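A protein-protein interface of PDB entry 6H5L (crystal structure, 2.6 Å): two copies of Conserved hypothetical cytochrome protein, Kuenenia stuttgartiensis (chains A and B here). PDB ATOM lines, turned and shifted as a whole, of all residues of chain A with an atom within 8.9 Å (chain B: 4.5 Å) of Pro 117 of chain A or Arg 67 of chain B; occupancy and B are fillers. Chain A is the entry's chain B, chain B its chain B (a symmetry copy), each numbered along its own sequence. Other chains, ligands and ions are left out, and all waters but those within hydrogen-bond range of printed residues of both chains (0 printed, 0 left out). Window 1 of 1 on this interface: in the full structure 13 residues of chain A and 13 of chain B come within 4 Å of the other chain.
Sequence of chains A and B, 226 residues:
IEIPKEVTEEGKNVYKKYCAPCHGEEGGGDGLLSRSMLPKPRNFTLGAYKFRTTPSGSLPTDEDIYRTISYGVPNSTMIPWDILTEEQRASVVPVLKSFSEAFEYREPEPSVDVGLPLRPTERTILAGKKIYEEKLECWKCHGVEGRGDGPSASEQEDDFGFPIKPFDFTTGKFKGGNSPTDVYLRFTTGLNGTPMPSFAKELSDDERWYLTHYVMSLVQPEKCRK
Among the printed residues, merely in contact across the chains: Leu 116 of chain A with Tyr 66 of chain B (3.6 Å), Leu 116 of chain A with Arg 67 of chain B (3.7 Å), Pro 117 of chain A with Arg 67 of chain B (3.9 Å), Pro 117 of chain A with Tyr 71 of chain B (3.3 Å), Arg 119 of chain A with Gly 72 of chain B (3.6 Å) and Pro 120 of chain A with Tyr 71 of chain B (3.8 Å).
The guanidinium group (NH1) of Arg 119 of chain A sits at hydrogen-bond distance from the backbone carbonyl oxygen (O) of Tyr 71 of chain B.
Of the 18 printed residues of chain A, 4 touch a printed residue of chain B. Printed residues of chain A that touch a printed residue of chain B: Leu 116, Pro 117, Arg 119 and Pro 120. Hydrophobic or aromatic side chains of chain A that line the printed part of chain B: Leu 116, Pro 117 and Pro 120. Hydrophobic or aromatic side chains of chain B within 4 Å of the printed part of chain A: Tyr 66 and Tyr 71. Among the printed residues, 7 pairs touch across the chains. Among the printed residues, no Asp or Glu carboxylate lies within 4 Å of a Lys or Arg side-chain nitrogen of the other chain.
Of chain B, only Arg 67 and Tyr 71 come within 4 Å of Pro 117 of chain A. Of the printed residues of chain B, Arg 119 of chain A touches Tyr 71 and Gly 72. Arg 67 of chain B touches just these residues of chain A: Leu 116 and Pro 117. Of the printed residues of chain A, Tyr 71 of chain B touches Pro 117 (3.3 Å), Arg 119 (2.8 Å) and Pro 120 (3.8 Å). Of the printed residues of chain A, Gly 72 of chain B touches Arg 119 (3.6 Å).
The backbone carbonyl oxygen (O) of Tyr 66 of chain B sits at hydrogen-bond distance from the side-chain hydroxyl (OG) of Ser 70 of chain B (3.0 Å).
No position is printed for both chains. Of the 7 pairs that touch across the chains among the printed residues, none has its exchanged pair printed and touching as well.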
ATOM      1  N   VAL A 114       3.063  19.617 -24.982  1.00  0.00           N
ATOM      2  CA  VAL A 114       2.307  19.208 -23.800  1.00  0.00           C
ATOM      3  C   VAL A 114       3.187  19.268 -22.559  1.00  0.00           C
ATOM      4  O   VAL A 114       2.799  19.825 -21.525  1.00  0.00           O
ATOM      5  CB  VAL A 114       1.718  17.800 -24.000  1.00  0.00           C
ATOM      6  CG1 VAL A 114       1.057  17.320 -22.718  1.00  0.00           C
ATOM      7  CG2 VAL A 114       0.733  17.795 -25.158  1.00  0.00           C
ATOM      8  N   GLY A 115       4.382  18.699 -22.644  1.00  0.00           N
ATOM      9  CA  GLY A 115       5.221  18.574 -21.476  1.00  0.00           C
ATOM     10  C   GLY A 115       4.869  17.330 -20.682  1.00  0.00           C
ATOM     11  O   GLY A 115       4.190  16.414 -21.157  1.00  0.00           O
ATOM     12  N   LEU A 116       5.337  17.307 -19.446  1.00  0.00           N
ATOM     13  CA  LEU A 116       5.083  16.151 -18.599  1.00  0.00           C
ATOM     14  C   LEU A 116       3.881  16.413 -17.709  1.00  0.00           C
ATOM     15  O   LEU A 116       3.852  17.433 -17.007  1.00  0.00           O
ATOM     16  CB  LEU A 116       6.307  15.845 -17.741  1.00  0.00           C
ATOM     17  CG  LEU A 116       7.629  15.761 -18.507  1.00  0.00           C
ATOM     18  CD1 LEU A 116       8.798  15.693 -17.542  1.00  0.00           C
ATOM     19  CD2 LEU A 116       7.629  14.561 -19.443  1.00  0.00           C
ATOM     20  N   PRO A 117       2.876  15.539 -17.714  1.00  0.00           N
ATOM     21  CA  PRO A 117       1.721  15.741 -16.829  1.00  0.00           C
ATOM     22  C   PRO A 117       2.133  15.698 -15.363  1.00  0.00           C
ATOM     23  O   PRO A 117       2.805  14.766 -14.917  1.00  0.00           O
ATOM     24  CB  PRO A 117       0.784  14.582 -17.195  1.00  0.00           C
ATOM     25  CG  PRO A 117       1.660  13.566 -17.858  1.00  0.00           C
ATOM     26  CD  PRO A 117       2.719  14.350 -18.568  1.00  0.00           C
ATOM     27  N   LEU A 118       1.728  16.724 -14.619  1.00  0.00           N
ATOM     28  CA  LEU A 118       2.073  16.817 -13.208  1.00  0.00           C
ATOM     29  C   LEU A 118       1.310  15.779 -12.393  1.00  0.00           C
ATOM     30  O   LEU A 118       0.210  15.352 -12.757  1.00  0.00           O
ATOM     31  CB  LEU A 118       1.778  18.219 -12.671  1.00  0.00           C
ATOM     32  CG  LEU A 118       2.923  19.235 -12.629  1.00  0.00           C
ATOM     33  CD1 LEU A 118       3.789  19.116 -13.867  1.00  0.00           C
ATOM     34  CD2 LEU A 118       2.380  20.651 -12.497  1.00  0.00           C
ATOM     35  N   ARG A 119       1.905  15.382 -11.278  1.00  0.00           N
ATOM     36  CA  ARG A 119       1.314  14.372 -10.406  1.00  0.00           C
ATOM     37  C   ARG A 119       0.121  14.952  -9.658  1.00  0.00           C
ATOM     38  O   ARG A 119       0.281  15.939  -8.924  1.00  0.00           O
ATOM     39  CB  ARG A 119       2.366  13.860  -9.427  1.00  0.00           C
ATOM     40  CG  ARG A 119       1.839  12.930  -8.351  1.00  0.00           C
ATOM     41  CD  ARG A 119       1.946  11.470  -8.761  1.00  0.00           C
ATOM     42  NE  ARG A 119       1.896  10.585  -7.599  1.00  0.00           N
ATOM     43  CZ  ARG A 119       2.969  10.151  -6.944  1.00  0.00           C
ATOM     44  NH1 ARG A 119       4.181  10.512  -7.340  1.00  0.00           N
ATOM     45  NH2 ARG A 119       2.831   9.354  -5.894  1.00  0.00           N
ATOM     46  N   PRO A 120      -1.078  14.393  -9.808  1.00  0.00           N
ATOM     47  CA  PRO A 120      -2.229  14.916  -9.063  1.00  0.00           C
ATOM     48  C   PRO A 120      -2.110  14.632  -7.574  1.00  0.00           C
ATOM     49  O   PRO A 120      -1.772  13.521  -7.158  1.00  0.00           O
ATOM     50  CB  PRO A 120      -3.419  14.173  -9.679  1.00  0.00           C
ATOM     51  CG  PRO A 120      -2.830  12.923 -10.251  1.00  0.00           C
ATOM     52  CD  PRO A 120      -1.452  13.298 -10.719  1.00  0.00           C
ATOM     53  N   SER A 179      -8.716  12.070 -21.548  1.00  0.00           N
ATOM     54  CA  SER A 179      -7.393  11.940 -20.962  1.00  0.00           C
ATOM     55  C   SER A 179      -7.003  13.223 -20.230  1.00  0.00           C
ATOM     56  O   SER A 179      -7.456  14.313 -20.592  1.00  0.00           O
ATOM     57  CB  SER A 179      -6.363  11.633 -22.046  1.00  0.00           C
ATOM     58  OG  SER A 179      -5.036  11.761 -21.559  1.00  0.00           O
ATOM     59  N   PRO A 180      -6.174  13.118 -19.188  1.00  0.00           N
ATOM     60  CA  PRO A 180      -5.643  14.340 -18.563  1.00  0.00           C
ATOM     61  C   PRO A 180      -4.847  15.200 -19.530  1.00  0.00           C
ATOM     62  O   PRO A 180      -4.864  16.432 -19.414  1.00  0.00           O
ATOM     63  CB  PRO A 180      -4.767  13.802 -17.423  1.00  0.00           C
ATOM     64  CG  PRO A 180      -5.310  12.439 -17.135  1.00  0.00           C
ATOM     65  CD  PRO A 180      -5.783  11.902 -18.454  1.00  0.00           C
ATOM     66  N   THR A 181      -4.149  14.582 -20.489  1.00  0.00           N
ATOM     67  CA  THR A 181      -3.479  15.351 -21.535  1.00  0.00           C
ATOM     68  C   THR A 181      -4.491  16.025 -22.452  1.00  0.00           C
ATOM     69  O   THR A 181      -4.282  17.162 -22.889  1.00  0.00           O
ATOM     70  CB  THR A 181      -2.545  14.443 -22.339  1.00  0.00           C
ATOM     71  OG1 THR A 181      -1.566  13.863 -21.466  1.00  0.00           O
ATOM     72  CG2 THR A 181      -1.839  15.229 -23.439  1.00  0.00           C
ATOM     73  N   ASP A 182      -5.598  15.338 -22.748  1.00  0.00           N
ATOM     74  CA  ASP A 182      -6.624  15.908 -23.616  1.00  0.00           C
ATOM     75  C   ASP A 182      -7.254  17.143 -22.983  1.00  0.00           C
ATOM     76  O   ASP A 182      -7.416  18.179 -23.640  1.00  0.00           O
ATOM     77  CB  ASP A 182      -7.691  14.856 -23.924  1.00  0.00           C
ATOM     78  CG  ASP A 182      -7.150  13.699 -24.738  1.00  0.00           C
ATOM     79  OD1 ASP A 182      -6.027  13.820 -25.273  1.00  0.00           O
ATOM     80  OD2 ASP A 182      -7.844  12.665 -24.836  1.00  0.00           O
ATOM     81  N   TYR A 184      -5.974  19.008 -20.587  1.00  0.00           N
ATOM     82  CA  TYR A 184      -4.945  20.042 -20.535  1.00  0.00           C
ATOM     83  C   TYR A 184      -4.779  20.718 -21.891  1.00  0.00           C
ATOM     84  O   TYR A 184      -4.535  21.929 -21.962  1.00  0.00           O
ATOM     85  CB  TYR A 184      -3.617  19.440 -20.069  1.00  0.00           C
ATOM     86  CG  TYR A 184      -2.429  20.368 -20.225  1.00  0.00           C
ATOM     87  CD1 TYR A 184      -2.127  21.310 -19.250  1.00  0.00           C
ATOM     88  CD2 TYR A 184      -1.609  20.295 -21.344  1.00  0.00           C
ATOM     89  CE1 TYR A 184      -1.042  22.158 -19.389  1.00  0.00           C
ATOM     90  CE2 TYR A 184      -0.524  21.139 -21.492  1.00  0.00           C
ATOM     91  CZ  TYR A 184      -0.246  22.068 -20.511  1.00  0.00           C
ATOM     92  OH  TYR A 184       0.833  22.910 -20.650  1.00  0.00           O
ATOM     93  N   ASP A 205       1.798  26.804 -17.471  1.00  0.00           N
ATOM     94  CA  ASP A 205       1.665  25.372 -17.723  1.00  0.00           C
ATOM     95  C   ASP A 205       1.274  24.623 -16.457  1.00  0.00           C
ATOM     96  O   ASP A 205       0.399  23.749 -16.489  1.00  0.00           O
ATOM     97  CB  ASP A 205       2.968  24.811 -18.292  1.00  0.00           C
ATOM     98  CG  ASP A 205       3.177  25.177 -19.747  1.00  0.00           C
ATOM     99  OD1 ASP A 205       2.275  25.811 -20.338  1.00  0.00           O
ATOM    100  OD2 ASP A 205       4.240  24.828 -20.304  1.00  0.00           O
ATOM    101  N   ASP A 206       1.901  24.960 -15.328  1.00  0.00           N
ATOM    102  CA  ASP A 206       1.607  24.262 -14.080  1.00  0.00           C
ATOM    103  C   ASP A 206       0.189  24.548 -13.602  1.00  0.00           C
ATOM    104  O   ASP A 206      -0.489  23.652 -13.086  1.00  0.00           O
ATOM    105  CB  ASP A 206       2.624  24.653 -13.008  1.00  0.00           C
ATOM    106  CG  ASP A 206       4.029  24.182 -13.339  1.00  0.00           C
ATOM    107  OD1 ASP A 206       4.528  24.519 -14.434  1.00  0.00           O
ATOM    108  OD2 ASP A 206       4.638  23.486 -12.499  1.00  0.00           O
ATOM    109  N   TRP A 209      -2.355  22.428 -15.324  1.00  0.00           N
ATOM    110  CA  TRP A 209      -2.393  21.072 -14.786  1.00  0.00           C
ATOM    111  C   TRP A 209      -3.136  21.038 -13.456  1.00  0.00           C
ATOM    112  O   TRP A 209      -3.875  20.087 -13.179  1.00  0.00           O
ATOM    113  CB  TRP A 209      -0.979  20.514 -14.628  1.00  0.00           C
ATOM    114  CG  TRP A 209      -0.333  20.123 -15.925  1.00  0.00           C
ATOM    115  CD1 TRP A 209       0.731  20.728 -16.526  1.00  0.00           C
ATOM    116  CD2 TRP A 209      -0.716  19.039 -16.784  1.00  0.00           C
ATOM    117  NE1 TRP A 209       1.037  20.089 -17.703  1.00  0.00           N
ATOM    118  CE2 TRP A 209       0.164  19.050 -17.885  1.00  0.00           C
ATOM    119  CE3 TRP A 209      -1.715  18.062 -16.729  1.00  0.00           C
ATOM    120  CZ2 TRP A 209       0.075  18.123 -18.922  1.00  0.00           C
ATOM    121  CZ3 TRP A 209      -1.802  17.142 -17.759  1.00  0.00           C
ATOM    122  CH2 TRP A 209      -0.913  17.179 -18.841  1.00  0.00           C
ATOM    123  N   TYR A 210      -2.943  22.061 -12.617  1.00  0.00           N
ATOM    124  CA  TYR A 210      -3.766  22.204 -11.418  1.00  0.00           C
ATOM    125  C   TYR A 210      -5.242  22.244 -11.786  1.00  0.00           C
ATOM    126  O   TYR A 210      -6.067  21.533 -11.198  1.00  0.00           O
ATOM    127  CB  TYR A 210      -3.395  23.477 -10.650  1.00  0.00           C
ATOM    128  CG  TYR A 210      -1.943  23.633 -10.248  1.00  0.00           C
ATOM    129  CD1 TYR A 210      -1.089  22.539 -10.171  1.00  0.00           C
ATOM    130  CD2 TYR A 210      -1.432  24.886  -9.932  1.00  0.00           C
ATOM    131  CE1 TYR A 210       0.237  22.696  -9.800  1.00  0.00           C
ATOM    132  CE2 TYR A 210      -0.114  25.051  -9.561  1.00  0.00           C
ATOM    133  CZ  TYR A 210       0.717  23.953  -9.495  1.00  0.00           C
ATOM    134  OH  TYR A 210       2.032  24.114  -9.125  1.00  0.00           O
ATOM    135  N   THR A 212      -6.653  21.218 -14.583  1.00  0.00           N
ATOM    136  CA  THR A 212      -7.043  19.923 -15.134  1.00  0.00           C
ATOM    137  C   THR A 212      -7.344  18.923 -14.026  1.00  0.00           C
ATOM    138  O   THR A 212      -8.338  18.191 -14.093  1.00  0.00           O
ATOM    139  CB  THR A 212      -5.943  19.387 -16.051  1.00  0.00           C
ATOM    140  OG1 THR A 212      -5.827  20.226 -17.206  1.00  0.00           O
ATOM    141  CG2 THR A 212      -6.251  17.968 -16.487  1.00  0.00           C
ATOM    142  N   HIS A 213      -6.499  18.884 -12.992  1.00  0.00           N
ATOM    143  CA  HIS A 213      -6.701  17.931 -11.904  1.00  0.00           C
ATOM    144  C   HIS A 213      -8.027  18.168 -11.194  1.00  0.00           C
ATOM    145  O   HIS A 213      -8.711  17.212 -10.810  1.00  0.00           O
ATOM    146  CB  HIS A 213      -5.538  18.011 -10.913  1.00  0.00           C
ATOM    147  CG  HIS A 213      -4.230  17.554 -11.482  1.00  0.00           C
ATOM    148  ND1 HIS A 213      -3.020  17.833 -10.883  1.00  0.00           N
ATOM    149  CD2 HIS A 213      -3.943  16.837 -12.595  1.00  0.00           C
ATOM    150  CE1 HIS A 213      -2.044  17.309 -11.602  1.00  0.00           C
ATOM    151  NE2 HIS A 213      -2.576  16.698 -12.646  1.00  0.00           N
ATOM    152  N   GLU B  63      14.990  10.569 -21.283  1.00  0.00           N
ATOM    153  CA  GLU B  63      13.711  11.211 -21.003  1.00  0.00           C
ATOM    154  C   GLU B  63      12.826  10.336 -20.125  1.00  0.00           C
ATOM    155  O   GLU B  63      12.066  10.857 -19.302  1.00  0.00           O
ATOM    156  CB  GLU B  63      12.996  11.543 -22.313  1.00  0.00           C
ATOM    157  CG  GLU B  63      13.776  12.475 -23.245  1.00  0.00           C
ATOM    158  CD  GLU B  63      14.899  11.769 -23.981  1.00  0.00           C
ATOM    159  OE1 GLU B  63      14.816  10.536 -24.152  1.00  0.00           O
ATOM    160  OE2 GLU B  63      15.871  12.446 -24.374  1.00  0.00           O
ATOM    161  N   ASP B  64      12.912   9.010 -20.279  1.00  0.00           N
ATOM    162  CA  ASP B  64      12.150   8.111 -19.418  1.00  0.00           C
ATOM    163  C   ASP B  64      12.541   8.291 -17.960  1.00  0.00           C
ATOM    164  O   ASP B  64      11.676   8.336 -17.077  1.00  0.00           O
ATOM    165  CB  ASP B  64      12.368   6.659 -19.847  1.00  0.00           C
ATOM    166  CG  ASP B  64      11.696   6.335 -21.165  1.00  0.00           C
ATOM    167  OD1 ASP B  64      10.886   7.157 -21.640  1.00  0.00           O
ATOM    168  OD2 ASP B  64      11.981   5.256 -21.729  1.00  0.00           O
ATOM    169  N   ILE B  65      13.843   8.385 -17.686  1.00  0.00           N
ATOM    170  CA  ILE B  65      14.308   8.545 -16.311  1.00  0.00           C
ATOM    171  C   ILE B  65      13.883   9.901 -15.760  1.00  0.00           C
ATOM    172  O   ILE B  65      13.381  10.002 -14.635  1.00  0.00           O
ATOM    173  CB  ILE B  65      15.833   8.354 -16.236  1.00  0.00           C
ATOM    174  CG1 ILE B  65      16.226   6.979 -16.780  1.00  0.00           C
ATOM    175  CG2 ILE B  65      16.324   8.523 -14.806  1.00  0.00           C
ATOM    176  CD1 ILE B  65      17.724   6.777 -16.899  1.00  0.00           C
ATOM    177  N   TYR B  66      14.076  10.964 -16.546  1.00  0.00           N
ATOM    178  CA  TYR B  66      13.664  12.296 -16.112  1.00  0.00           C
ATOM    179  C   TYR B  66      12.170  12.353 -15.824  1.00  0.00           C
ATOM    180  O   TYR B  66      11.740  13.076 -14.919  1.00  0.00           O
ATOM    181  CB  TYR B  66      14.039  13.330 -17.175  1.00  0.00           C
ATOM    182  CG  TYR B  66      13.712  14.755 -16.793  1.00  0.00           C
ATOM    183  CD1 TYR B  66      14.631  15.540 -16.109  1.00  0.00           C
ATOM    184  CD2 TYR B  66      12.481  15.316 -17.114  1.00  0.00           C
ATOM    185  CE1 TYR B  66      14.333  16.842 -15.754  1.00  0.00           C
ATOM    186  CE2 TYR B  66      12.174  16.615 -16.761  1.00  0.00           C
ATOM    187  CZ  TYR B  66      13.103  17.372 -16.082  1.00  0.00           C
ATOM    188  OH  TYR B  66      12.795  18.663 -15.732  1.00  0.00           O
ATOM    189  N   ARG B  67      11.365  11.603 -16.578  1.00  0.00           N
ATOM    190  CA  ARG B  67       9.926  11.597 -16.344  1.00  0.00           C
ATOM    191  C   ARG B  67       9.594  10.948 -15.008  1.00  0.00           C
ATOM    192  O   ARG B  67       8.781  11.474 -14.239  1.00  0.00           O
ATOM    193  CB  ARG B  67       9.216  10.875 -17.486  1.00  0.00           C
ATOM    194  CG  ARG B  67       7.700  10.991 -17.446  1.00  0.00           C
ATOM    195  CD  ARG B  67       7.063  10.325 -18.656  1.00  0.00           C
ATOM    196  NE  ARG B  67       6.048  11.176 -19.268  1.00  0.00           N
ATOM    197  CZ  ARG B  67       5.260  10.799 -20.269  1.00  0.00           C
ATOM    198  NH1 ARG B  67       5.365   9.577 -20.774  1.00  0.00           N
ATOM    199  NH2 ARG B  67       4.366  11.644 -20.762  1.00  0.00           N
ATOM    200  N   THR B  68      10.210   9.800 -14.717  1.00  0.00           N
ATOM    201  CA  THR B  68       9.945   9.114 -13.455  1.00  0.00           C
ATOM    202  C   THR B  68      10.386   9.957 -12.263  1.00  0.00           C
ATOM    203  O   THR B  68       9.711   9.980 -11.227  1.00  0.00           O
ATOM    204  CB  THR B  68      10.649   7.757 -13.439  1.00  0.00           C
ATOM    205  OG1 THR B  68      10.358   7.053 -14.655  1.00  0.00           O
ATOM    206  CG2 THR B  68      10.177   6.922 -12.260  1.00  0.00           C
ATOM    207  N   ILE B  69      11.518  10.654 -12.393  1.00  0.00           N
ATOM    208  CA  ILE B  69      11.992  11.527 -11.321  1.00  0.00           C
ATOM    209  C   ILE B  69      11.000  12.657 -11.073  1.00  0.00           C
ATOM    210  O   ILE B  69      10.684  12.986  -9.924  1.00  0.00           O
ATOM    211  CB  ILE B  69      13.393  12.072 -11.660  1.00  0.00           C
ATOM    212  CG1 ILE B  69      14.394  10.927 -11.830  1.00  0.00           C
ATOM    213  CG2 ILE B  69      13.863  13.043 -10.589  1.00  0.00           C
ATOM    214  CD1 ILE B  69      15.707  11.352 -12.464  1.00  0.00           C
ATOM    215  N   SER B  70      10.487  13.261 -12.147  1.00  0.00           N
ATOM    216  CA  SER B  70       9.574  14.389 -12.000  1.00  0.00           C
ATOM    217  C   SER B  70       8.219  13.946 -11.467  1.00  0.00           C
ATOM    218  O   SER B  70       7.646  14.598 -10.586  1.00  0.00           O
ATOM    219  CB  SER B  70       9.412  15.106 -13.340  1.00  0.00           C
ATOM    220  OG  SER B  70      10.653  15.620 -13.792  1.00  0.00           O
ATOM    221  N   TYR B  71       7.687  12.840 -11.987  1.00  0.00           N
ATOM    222  CA  TYR B  71       6.343  12.416 -11.613  1.00  0.00           C
ATOM    223  C   TYR B  71       6.330  11.616 -10.317  1.00  0.00           C
ATOM    224  O   TYR B  71       5.340  11.663  -9.577  1.00  0.00           O
ATOM    225  CB  TYR B  71       5.727  11.596 -12.746  1.00  0.00           C
ATOM    226  CG  TYR B  71       4.276  11.227 -12.552  1.00  0.00           C
ATOM    227  CD1 TYR B  71       3.263  12.072 -12.981  1.00  0.00           C
ATOM    228  CD2 TYR B  71       3.919  10.022 -11.960  1.00  0.00           C
ATOM    229  CE1 TYR B  71       1.936  11.736 -12.817  1.00  0.00           C
ATOM    230  CE2 TYR B  71       2.592   9.676 -11.792  1.00  0.00           C
ATOM    231  CZ  TYR B  71       1.605  10.538 -12.223  1.00  0.00           C
ATOM    232  OH  TYR B  71       0.280  10.209 -12.065  1.00  0.00           O
ATOM    233  N   GLY B  72       7.404  10.888 -10.024  1.00  0.00           N
ATOM    234  CA  GLY B  72       7.424  10.003  -8.880  1.00  0.00           C
ATOM    235  C   GLY B  72       6.769   8.674  -9.197  1.00  0.00           C
ATOM    236  O   GLY B  72       6.295   8.417 -10.306  1.00  0.00           O
